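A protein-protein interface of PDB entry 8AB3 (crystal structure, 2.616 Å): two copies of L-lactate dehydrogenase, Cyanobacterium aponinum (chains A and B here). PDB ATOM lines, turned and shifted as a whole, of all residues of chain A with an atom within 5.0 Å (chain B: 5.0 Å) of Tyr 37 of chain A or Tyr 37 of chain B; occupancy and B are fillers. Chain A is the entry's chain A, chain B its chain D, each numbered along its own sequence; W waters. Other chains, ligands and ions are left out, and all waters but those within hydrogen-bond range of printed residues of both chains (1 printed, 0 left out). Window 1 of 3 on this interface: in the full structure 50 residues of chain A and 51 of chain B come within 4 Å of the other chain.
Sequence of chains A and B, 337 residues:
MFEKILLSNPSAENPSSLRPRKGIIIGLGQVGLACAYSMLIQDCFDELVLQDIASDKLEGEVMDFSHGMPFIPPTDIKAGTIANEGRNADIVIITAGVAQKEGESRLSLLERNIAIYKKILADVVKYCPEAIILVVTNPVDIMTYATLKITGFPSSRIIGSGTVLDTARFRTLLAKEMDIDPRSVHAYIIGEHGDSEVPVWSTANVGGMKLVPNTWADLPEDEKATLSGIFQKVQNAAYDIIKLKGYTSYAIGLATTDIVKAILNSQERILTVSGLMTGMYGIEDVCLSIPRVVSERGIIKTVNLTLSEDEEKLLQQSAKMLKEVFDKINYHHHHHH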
ATOM      1  N   LEU A  33       1.935  25.345  21.464  1.00  0.00           N
ATOM      2  CA  LEU A  33       0.927  24.970  20.463  1.00  0.00           C
ATOM      3  C   LEU A  33       1.034  23.506  20.067  1.00  0.00           C
ATOM      4  O   LEU A  33       0.005  22.825  19.961  1.00  0.00           O
ATOM      5  CB  LEU A  33       0.954  25.872  19.234  1.00  0.00           C
ATOM      6  CG  LEU A  33       0.445  27.290  19.468  1.00  0.00           C
ATOM      7  CD1 LEU A  33       0.751  28.183  18.292  1.00  0.00           C
ATOM      8  CD2 LEU A  33      -1.025  27.290  19.858  1.00  0.00           C
ATOM      9  N   ALA A  34       2.276  22.988  19.951  1.00  0.00           N
ATOM     10  CA  ALA A  34       2.491  21.580  19.614  1.00  0.00           C
ATOM     11  C   ALA A  34       1.945  20.695  20.728  1.00  0.00           C
ATOM     12  O   ALA A  34       1.301  19.686  20.435  1.00  0.00           O
ATOM     13  CB  ALA A  34       3.966  21.300  19.386  1.00  0.00           C
ATOM     14  N   CYS A  35       2.136  21.114  22.007  1.00  0.00           N
ATOM     15  CA  CYS A  35       1.616  20.405  23.176  1.00  0.00           C
ATOM     16  C   CYS A  35       0.107  20.396  23.104  1.00  0.00           C
ATOM     17  O   CYS A  35      -0.492  19.335  23.207  1.00  0.00           O
ATOM     18  CB  CYS A  35       2.097  21.039  24.480  1.00  0.00           C
ATOM     19  SG  CYS A  35       3.859  20.809  24.826  1.00  0.00           S
ATOM     20  N   ALA A  36      -0.519  21.562  22.900  1.00  0.00           N
ATOM     21  CA  ALA A  36      -1.975  21.651  22.829  1.00  0.00           C
ATOM     22  C   ALA A  36      -2.570  20.756  21.715  1.00  0.00           C
ATOM     23  O   ALA A  36      -3.509  20.010  21.973  1.00  0.00           O
ATOM     24  CB  ALA A  36      -2.409  23.101  22.647  1.00  0.00           C
ATOM     25  N   TYR A  37      -1.994  20.797  20.507  1.00  0.00           N
ATOM     26  CA  TYR A  37      -2.466  19.984  19.379  1.00  0.00           C
ATOM     27  C   TYR A  37      -2.393  18.502  19.697  1.00  0.00           C
ATOM     28  O   TYR A  37      -3.399  17.808  19.545  1.00  0.00           O
ATOM     29  CB  TYR A  37      -1.644  20.294  18.109  1.00  0.00           C
ATOM     30  CG  TYR A  37      -2.356  19.988  16.813  1.00  0.00           C
ATOM     31  CD1 TYR A  37      -3.730  20.181  16.683  1.00  0.00           C
ATOM     32  CD2 TYR A  37      -1.647  19.581  15.688  1.00  0.00           C
ATOM     33  CE1 TYR A  37      -4.380  19.953  15.472  1.00  0.00           C
ATOM     34  CE2 TYR A  37      -2.286  19.355  14.471  1.00  0.00           C
ATOM     35  CZ  TYR A  37      -3.651  19.556  14.363  1.00  0.00           C
ATOM     36  OH  TYR A  37      -4.262  19.361  13.149  1.00  0.00           O
ATOM     37  N   SER A  38      -1.218  18.014  20.159  1.00  0.00           N
ATOM     38  CA  SER A  38      -1.029  16.606  20.497  1.00  0.00           C
ATOM     39  C   SER A  38      -1.967  16.165  21.621  1.00  0.00           C
ATOM     40  O   SER A  38      -2.606  15.121  21.500  1.00  0.00           O
ATOM     41  CB  SER A  38       0.434  16.327  20.861  1.00  0.00           C
ATOM     42  OG  SER A  38       0.610  15.055  21.465  1.00  0.00           O
ATOM     43  N   MET A  39      -2.060  16.955  22.696  1.00  0.00           N
ATOM     44  CA  MET A  39      -2.912  16.635  23.841  1.00  0.00           C
ATOM     45  C   MET A  39      -4.403  16.608  23.483  1.00  0.00           C
ATOM     46  O   MET A  39      -5.169  15.920  24.157  1.00  0.00           O
ATOM     47  CB  MET A  39      -2.626  17.578  25.037  1.00  0.00           C
ATOM     48  CG  MET A  39      -1.297  17.304  25.703  1.00  0.00           C
ATOM     49  SD  MET A  39      -0.716  18.614  26.800  1.00  0.00           S
ATOM     50  CE  MET A  39       0.969  18.116  27.060  1.00  0.00           C
ATOM     51  N   LEU A  40      -4.816  17.337  22.435  1.00  0.00           N
ATOM     52  CA  LEU A  40      -6.211  17.318  22.012  1.00  0.00           C
ATOM     53  C   LEU A  40      -6.470  16.071  21.167  1.00  0.00           C
ATOM     54  O   LEU A  40      -7.476  15.393  21.382  1.00  0.00           O
ATOM     55  CB  LEU A  40      -6.577  18.563  21.197  1.00  0.00           C
ATOM     56  CG  LEU A  40      -6.702  19.858  21.963  1.00  0.00           C
ATOM     57  CD1 LEU A  40      -6.742  21.034  21.017  1.00  0.00           C
ATOM     58  CD2 LEU A  40      -7.891  19.839  22.911  1.00  0.00           C
ATOM     59  N   ILE A  41      -5.575  15.769  20.198  1.00  0.00           N
ATOM     60  CA  ILE A  41      -5.720  14.596  19.329  1.00  0.00           C
ATOM     61  C   ILE A  41      -5.662  13.294  20.150  1.00  0.00           C
ATOM     62  O   ILE A  41      -6.393  12.356  19.856  1.00  0.00           O
ATOM     63  CB  ILE A  41      -4.655  14.620  18.190  1.00  0.00           C
ATOM     64  CG1 ILE A  41      -4.863  15.808  17.241  1.00  0.00           C
ATOM     65  CG2 ILE A  41      -4.606  13.302  17.417  1.00  0.00           C
ATOM     66  CD1 ILE A  41      -3.667  16.042  16.314  1.00  0.00           C
ATOM     67  N   PHE A  65      -8.383  25.570  17.201  1.00  0.00           N
ATOM     68  CA  PHE A  65      -8.392  24.306  17.924  1.00  0.00           C
ATOM     69  C   PHE A  65      -9.808  23.795  18.101  1.00  0.00           C
ATOM     70  O   PHE A  65     -10.062  22.620  17.849  1.00  0.00           O
ATOM     71  CB  PHE A  65      -7.700  24.431  19.293  1.00  0.00           C
ATOM     72  CG  PHE A  65      -6.195  24.335  19.268  1.00  0.00           C
ATOM     73  CD1 PHE A  65      -5.555  23.372  18.506  1.00  0.00           C
ATOM     74  CD2 PHE A  65      -5.419  25.184  20.037  1.00  0.00           C
ATOM     75  CE1 PHE A  65      -4.163  23.266  18.512  1.00  0.00           C
ATOM     76  CE2 PHE A  65      -4.032  25.086  20.025  1.00  0.00           C
ATOM     77  CZ  PHE A  65      -3.413  24.119  19.275  1.00  0.00           C
ATOM     78  N   SER A 249       9.688  22.031  18.054  1.00  0.00           N
ATOM     79  CA  SER A 249       8.353  21.992  18.662  1.00  0.00           C
ATOM     80  C   SER A 249       7.661  20.618  18.679  1.00  0.00           C
ATOM     81  O   SER A 249       7.070  20.245  19.698  1.00  0.00           O
ATOM     82  CB  SER A 249       7.437  23.010  17.987  1.00  0.00           C
ATOM     83  OG  SER A 249       7.262  22.724  16.607  1.00  0.00           O
ATOM     84  N   TYR A 250       7.681  19.900  17.554  1.00  0.00           N
ATOM     85  CA  TYR A 250       6.991  18.618  17.394  1.00  0.00           C
ATOM     86  C   TYR A 250       7.416  17.516  18.362  1.00  0.00           C
ATOM     87  O   TYR A 250       6.550  16.923  18.999  1.00  0.00           O
ATOM     88  CB  TYR A 250       7.101  18.130  15.950  1.00  0.00           C
ATOM     89  CG  TYR A 250       6.519  19.142  15.005  1.00  0.00           C
ATOM     90  CD1 TYR A 250       5.238  19.634  15.191  1.00  0.00           C
ATOM     91  CD2 TYR A 250       7.280  19.685  13.988  1.00  0.00           C
ATOM     92  CE1 TYR A 250       4.705  20.601  14.349  1.00  0.00           C
ATOM     93  CE2 TYR A 250       6.758  20.640  13.131  1.00  0.00           C
ATOM     94  CZ  TYR A 250       5.470  21.102  13.317  1.00  0.00           C
ATOM     95  OH  TYR A 250       4.965  22.072  12.479  1.00  0.00           O
ATOM     96  N   ALA A 251       8.717  17.217  18.467  1.00  0.00           N
ATOM     97  CA  ALA A 251       9.188  16.160  19.350  1.00  0.00           C
ATOM     98  C   ALA A 251       8.977  16.494  20.824  1.00  0.00           C
ATOM     99  O   ALA A 251       8.615  15.599  21.589  1.00  0.00           O
ATOM    100  CB  ALA A 251      10.643  15.847  19.070  1.00  0.00           C
ATOM    101  N   GLY A 253       6.561  18.403  21.993  1.00  0.00           N
ATOM    102  CA  GLY A 253       5.120  18.327  22.189  1.00  0.00           C
ATOM    103  C   GLY A 253       4.698  16.901  22.466  1.00  0.00           C
ATOM    104  O   GLY A 253       3.870  16.664  23.341  1.00  0.00           O
ATOM    105  N   LEU A 254       5.303  15.932  21.764  1.00  0.00           N
ATOM    106  CA  LEU A 254       5.026  14.511  22.000  1.00  0.00           C
ATOM    107  C   LEU A 254       5.670  14.003  23.308  1.00  0.00           C
ATOM    108  O   LEU A 254       5.063  13.190  23.998  1.00  0.00           O
ATOM    109  CB  LEU A 254       5.490  13.646  20.814  1.00  0.00           C
ATOM    110  CG  LEU A 254       4.715  13.809  19.504  1.00  0.00           C
ATOM    111  CD1 LEU A 254       5.294  12.928  18.423  1.00  0.00           C
ATOM    112  CD2 LEU A 254       3.257  13.497  19.694  1.00  0.00           C
ATOM    113  N   LEU B  33       2.210  21.265   7.472  1.00  0.00           N
ATOM    114  CA  LEU B  33       2.819  20.807   8.723  1.00  0.00           C
ATOM    115  C   LEU B  33       1.795  20.371   9.776  1.00  0.00           C
ATOM    116  O   LEU B  33       2.109  19.525  10.615  1.00  0.00           O
ATOM    117  CB  LEU B  33       3.784  21.845   9.276  1.00  0.00           C
ATOM    118  CG  LEU B  33       5.055  22.004   8.454  1.00  0.00           C
ATOM    119  CD1 LEU B  33       5.750  23.317   8.761  1.00  0.00           C
ATOM    120  CD2 LEU B  33       5.994  20.827   8.690  1.00  0.00           C
ATOM    121  N   ALA B  34       0.576  20.923   9.731  1.00  0.00           N
ATOM    122  CA  ALA B  34      -0.476  20.478  10.643  1.00  0.00           C
ATOM    123  C   ALA B  34      -0.980  19.112  10.177  1.00  0.00           C
ATOM    124  O   ALA B  34      -1.211  18.233  11.010  1.00  0.00           O
ATOM    125  CB  ALA B  34      -1.614  21.469  10.669  1.00  0.00           C
ATOM    126  N   CYS B  35      -1.101  18.911   8.840  1.00  0.00           N
ATOM    127  CA  CYS B  35      -1.486  17.642   8.238  1.00  0.00           C
ATOM    128  C   CYS B  35      -0.457  16.594   8.607  1.00  0.00           C
ATOM    129  O   CYS B  35      -0.837  15.555   9.116  1.00  0.00           O
ATOM    130  CB  CYS B  35      -1.621  17.765   6.720  1.00  0.00           C
ATOM    131  SG  CYS B  35      -3.028  18.761   6.165  1.00  0.00           S
ATOM    132  N   ALA B  36       0.838  16.866   8.394  1.00  0.00           N
ATOM    133  CA  ALA B  36       1.899  15.910   8.725  1.00  0.00           C
ATOM    134  C   ALA B  36       1.892  15.500  10.205  1.00  0.00           C
ATOM    135  O   ALA B  36       1.933  14.309  10.496  1.00  0.00           O
ATOM    136  CB  ALA B  36       3.254  16.473   8.336  1.00  0.00           C
ATOM    137  N   TYR B  37       1.773  16.465  11.129  1.00  0.00           N
ATOM    138  CA  TYR B  37       1.750  16.191  12.564  1.00  0.00           C
ATOM    139  C   TYR B  37       0.583  15.303  12.933  1.00  0.00           C
ATOM    140  O   TYR B  37       0.803  14.274  13.571  1.00  0.00           O
ATOM    141  CB  TYR B  37       1.691  17.496  13.357  1.00  0.00           C
ATOM    142  CG  TYR B  37       2.230  17.414  14.768  1.00  0.00           C
ATOM    143  CD1 TYR B  37       3.310  16.598  15.077  1.00  0.00           C
ATOM    144  CD2 TYR B  37       1.718  18.223  15.775  1.00  0.00           C
ATOM    145  CE1 TYR B  37       3.830  16.545  16.371  1.00  0.00           C
ATOM    146  CE2 TYR B  37       2.230  18.181  17.067  1.00  0.00           C
ATOM    147  CZ  TYR B  37       3.298  17.355  17.357  1.00  0.00           C
ATOM    148  OH  TYR B  37       3.823  17.363  18.626  1.00  0.00           O
ATOM    149  N   SER B  38      -0.651  15.665  12.512  1.00  0.00           N
ATOM    150  CA  SER B  38      -1.847  14.876  12.799  1.00  0.00           C
ATOM    151  C   SER B  38      -1.768  13.467  12.207  1.00  0.00           C
ATOM    152  O   SER B  38      -2.054  12.501  12.913  1.00  0.00           O
ATOM    153  CB  SER B  38      -3.105  15.592  12.304  1.00  0.00           C
ATOM    154  OG  SER B  38      -4.245  14.741  12.283  1.00  0.00           O
ATOM    155  N   MET B  39      -1.367  13.350  10.925  1.00  0.00           N
ATOM    156  CA  MET B  39      -1.248  12.064  10.239  1.00  0.00           C
ATOM    157  C   MET B  39      -0.185  11.157  10.872  1.00  0.00           C
ATOM    158  O   MET B  39      -0.287   9.941  10.747  1.00  0.00           O
ATOM    159  CB  MET B  39      -1.008  12.261   8.733  1.00  0.00           C
ATOM    160  CG  MET B  39      -2.235  12.751   7.999  1.00  0.00           C
ATOM    161  SD  MET B  39      -1.898  13.420   6.335  1.00  0.00           S
ATOM    162  CE  MET B  39      -3.458  14.200   5.993  1.00  0.00           C
ATOM    163  N   LEU B  40       0.823  11.732  11.559  1.00  0.00           N
ATOM    164  CA  LEU B  40       1.830  10.917  12.244  1.00  0.00           C
ATOM    165  C   LEU B  40       1.287  10.425  13.573  1.00  0.00           C
ATOM    166  O   LEU B  40       1.437   9.250  13.887  1.00  0.00           O
ATOM    167  CB  LEU B  40       3.131  11.695  12.486  1.00  0.00           C
ATOM    168  CG  LEU B  40       3.981  11.977  11.265  1.00  0.00           C
ATOM    169  CD1 LEU B  40       5.052  12.999  11.584  1.00  0.00           C
ATOM    170  CD2 LEU B  40       4.547  10.697  10.682  1.00  0.00           C
ATOM    171  N   ILE B  41       0.662  11.325  14.363  1.00  0.00           N
ATOM    172  CA  ILE B  41       0.095  10.971  15.672  1.00  0.00           C
ATOM    173  C   ILE B  41      -1.039   9.937  15.523  1.00  0.00           C
ATOM    174  O   ILE B  41      -1.171   9.043  16.339  1.00  0.00           O
ATOM    175  CB  ILE B  41      -0.361  12.253  16.441  1.00  0.00           C
ATOM    176  CG1 ILE B  41       0.834  13.169  16.792  1.00  0.00           C
ATOM    177  CG2 ILE B  41      -1.175  11.925  17.688  1.00  0.00           C
ATOM    178  CD1 ILE B  41       0.444  14.546  17.224  1.00  0.00           C
ATOM    179  N   PHE B  65      10.157  16.026  13.273  1.00  0.00           N
ATOM    180  CA  PHE B  65       9.115  15.009  13.197  1.00  0.00           C
ATOM    181  C   PHE B  65       9.658  13.646  13.572  1.00  0.00           C
ATOM    182  O   PHE B  65       9.049  12.947  14.375  1.00  0.00           O
ATOM    183  CB  PHE B  65       8.480  14.961  11.806  1.00  0.00           C
ATOM    184  CG  PHE B  65       7.408  15.992  11.537  1.00  0.00           C
ATOM    185  CD1 PHE B  65       6.420  16.242  12.465  1.00  0.00           C
ATOM    186  CD2 PHE B  65       7.344  16.650  10.320  1.00  0.00           C
ATOM    187  CE1 PHE B  65       5.405  17.146  12.195  1.00  0.00           C
ATOM    188  CE2 PHE B  65       6.331  17.560  10.055  1.00  0.00           C
ATOM    189  CZ  PHE B  65       5.364  17.798  10.992  1.00  0.00           C
ATOM    190  N   SER B 249      -4.657  26.512  10.431  1.00  0.00           N
ATOM    191  CA  SER B 249      -3.912  25.278  10.169  1.00  0.00           C
ATOM    192  C   SER B 249      -4.430  24.021  10.895  1.00  0.00           C
ATOM    193  O   SER B 249      -4.519  22.953  10.285  1.00  0.00           O
ATOM    194  CB  SER B 249      -2.431  25.490  10.473  1.00  0.00           C
ATOM    195  OG  SER B 249      -2.216  25.813  11.838  1.00  0.00           O
ATOM    196  N   TYR B 250      -4.718  24.133  12.194  1.00  0.00           N
ATOM    197  CA  TYR B 250      -5.121  23.012  13.038  1.00  0.00           C
ATOM    198  C   TYR B 250      -6.402  22.287  12.621  1.00  0.00           C
ATOM    199  O   TYR B 250      -6.375  21.064  12.494  1.00  0.00           O
ATOM    200  CB  TYR B 250      -5.210  23.472  14.491  1.00  0.00           C
ATOM    201  CG  TYR B 250      -3.862  23.948  14.959  1.00  0.00           C
ATOM    202  CD1 TYR B 250      -2.738  23.150  14.816  1.00  0.00           C
ATOM    203  CD2 TYR B 250      -3.687  25.234  15.436  1.00  0.00           C
ATOM    204  CE1 TYR B 250      -1.485  23.594  15.201  1.00  0.00           C
ATOM    205  CE2 TYR B 250      -2.436  25.692  15.818  1.00  0.00           C
ATOM    206  CZ  TYR B 250      -1.338  24.866  15.700  1.00  0.00           C
ATOM    207  OH  TYR B 250      -0.089  25.298  16.057  1.00  0.00           O
ATOM    208  N   ALA B 251      -7.511  23.012  12.406  1.00  0.00           N
ATOM    209  CA  ALA B 251      -8.766  22.374  12.014  1.00  0.00           C
ATOM    210  C   ALA B 251      -8.705  21.767  10.615  1.00  0.00           C
ATOM    211  O   ALA B 251      -9.251  20.690  10.417  1.00  0.00           O
ATOM    212  CB  ALA B 251      -9.913  23.350  12.131  1.00  0.00           C
ATOM    213  N   GLY B 253      -5.980  20.579   9.209  1.00  0.00           N
ATOM    214  CA  GLY B 253      -5.101  19.429   9.366  1.00  0.00           C
ATOM    215  C   GLY B 253      -5.886  18.219   9.826  1.00  0.00           C
ATOM    216  O   GLY B 253      -5.682  17.113   9.322  1.00  0.00           O
ATOM    217  N   LEU B 254      -6.845  18.427  10.739  1.00  0.00           N
ATOM    218  CA  LEU B 254      -7.705  17.342  11.219  1.00  0.00           C
ATOM    219  C   LEU B 254      -8.752  16.939  10.163  1.00  0.00           C
ATOM    220  O   LEU B 254      -9.052  15.749  10.034  1.00  0.00           O
ATOM    221  CB  LEU B 254      -8.402  17.722  12.539  1.00  0.00           C
ATOM    222  CG  LEU B 254      -7.516  17.832  13.775  1.00  0.00           C
ATOM    223  CD1 LEU B 254      -8.326  18.248  14.979  1.00  0.00           C
ATOM    224  CD2 LEU B 254      -6.768  16.541  14.041  1.00  0.00           C
HETATM  225  O   HOH W   1       7.944  14.710  16.366  1.00  0.00           O
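The side-chain hydroxyl of Tyr 37 of chain A sits at hydrogen-bond distance from the backbone carbonyl oxygen of Tyr 250 of chain B, 2.8 Å away. The backbone carbonyl oxygen (O) of Tyr 250 of chain A lies within hydrogen-bond range of the side-chain hydroxyl (OH) of Tyr 37 of chain B (2.8 Å).
CB of Leu 33 of chain A touches OH of Tyr 250 of chain B, 3.4 Å away. Tyr 37 of chain B touches Ala 34 of chain A (CE2 to O, 3.8 Å). Tyr 37 of chain A touches Tyr 37 of chain B (CD2 to CD2, 3.6 Å). C of Gly 253 of chain B touches OH of Tyr 37 of chain A (3.9 Å). Tyr 37 of chain A touches Leu 254 of chain B. Ile 41 of chain A touches Ile 41 of chain B (CG2 to CG2, 3.7 Å). Tyr 250 of chain A touches Leu 33 of chain B. Tyr 250 of chain A touches Phe 65 of chain B. Gly 253 of chain A touches Tyr 37 of chain B. Tyr 37 of chain B touches Leu 254 of chain A.
Of the printed residues of chain B, Ala 34 of chain A touches Tyr 37 (3.8 Å). Tyr 37 of chain A touches just these residues of chain B: Ala 34, Tyr 37, Tyr 250, Gly 253 and Leu 254. Printed residues of chain A within 4 Å of Ala 34 of chain B: Tyr 37. Tyr 37 of chain B touches just these residues of chain A: Ala 34, Tyr 37, Tyr 250, Gly 253 and Leu 254. Printed residues of chain A within 4 Å of Ile 41 of chain B: Ile 41 (3.7 Å) and Leu 254 (3.8 Å). Ser 249 of chain B touches none of the printed residues of chain A. Of the printed residues of chain A, Gly 253 of chain B touches Tyr 37. The nearest residue of chain A that does not touch Tyr 37 of chain B is Ser 38 of chain A (4.2 Å). The nearest printed residue of chain B that does not touch Ile 41 of chain A is Ser 38 of chain B (4.1 Å).
Printed residues of chain A that touch a printed residue of chain B: Leu 33, Ala 34, Tyr 37, Ile 41, Phe 65, Tyr 250, Gly 253 and Leu 254. Hydrophobic or aromatic side chains of chain A within 4 Å of the printed part of chain B: Leu 33, Tyr 37, Ile 41, Phe 65, Tyr 250 and Leu 254. Of the 15 printed residues of chain B, 8 touch a printed residue of chain A. Hydrophobic or aromatic side chains of chain B that line the printed part of chain A: Leu 33, Tyr 37, Ile 41, Phe 65, Tyr 250 and Leu 254. Along chain B the printed residues that touch a printed residue of chain A span positions 33 to 254. Among the printed residues, 16 pairs touch across the chains. Among the printed residues, no Asp or Glu carboxylate lies within 4 Å of a Lys or Arg side-chain nitrogen of the other chain.
Tyr 37 of chain B touches its own counterpart, Tyr 37 of chain A. Tyr 37 of chain A touches Tyr 250 of chain B, and with the chains exchanged Tyr 250 of chain A touches Tyr 37 of chain B. Tyr 37 of chain A touches Gly 253 of chain B, and with the chains exchanged Gly 253 of chain A touches Tyr 37 of chain B. Tyr 37 of chain A touches Leu 254 of chain B, and with the chains exchanged Leu 254 of chain A touches Tyr 37 of chain B. Of the 16 pairs that touch across the chains among the printed residues, 16 have their exchanged pair printed and touching as well.
Water W1 bridges O of Phe 65 of chain B (2.9 Å) and N of Ala 251 of chain A (3.4 Å).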
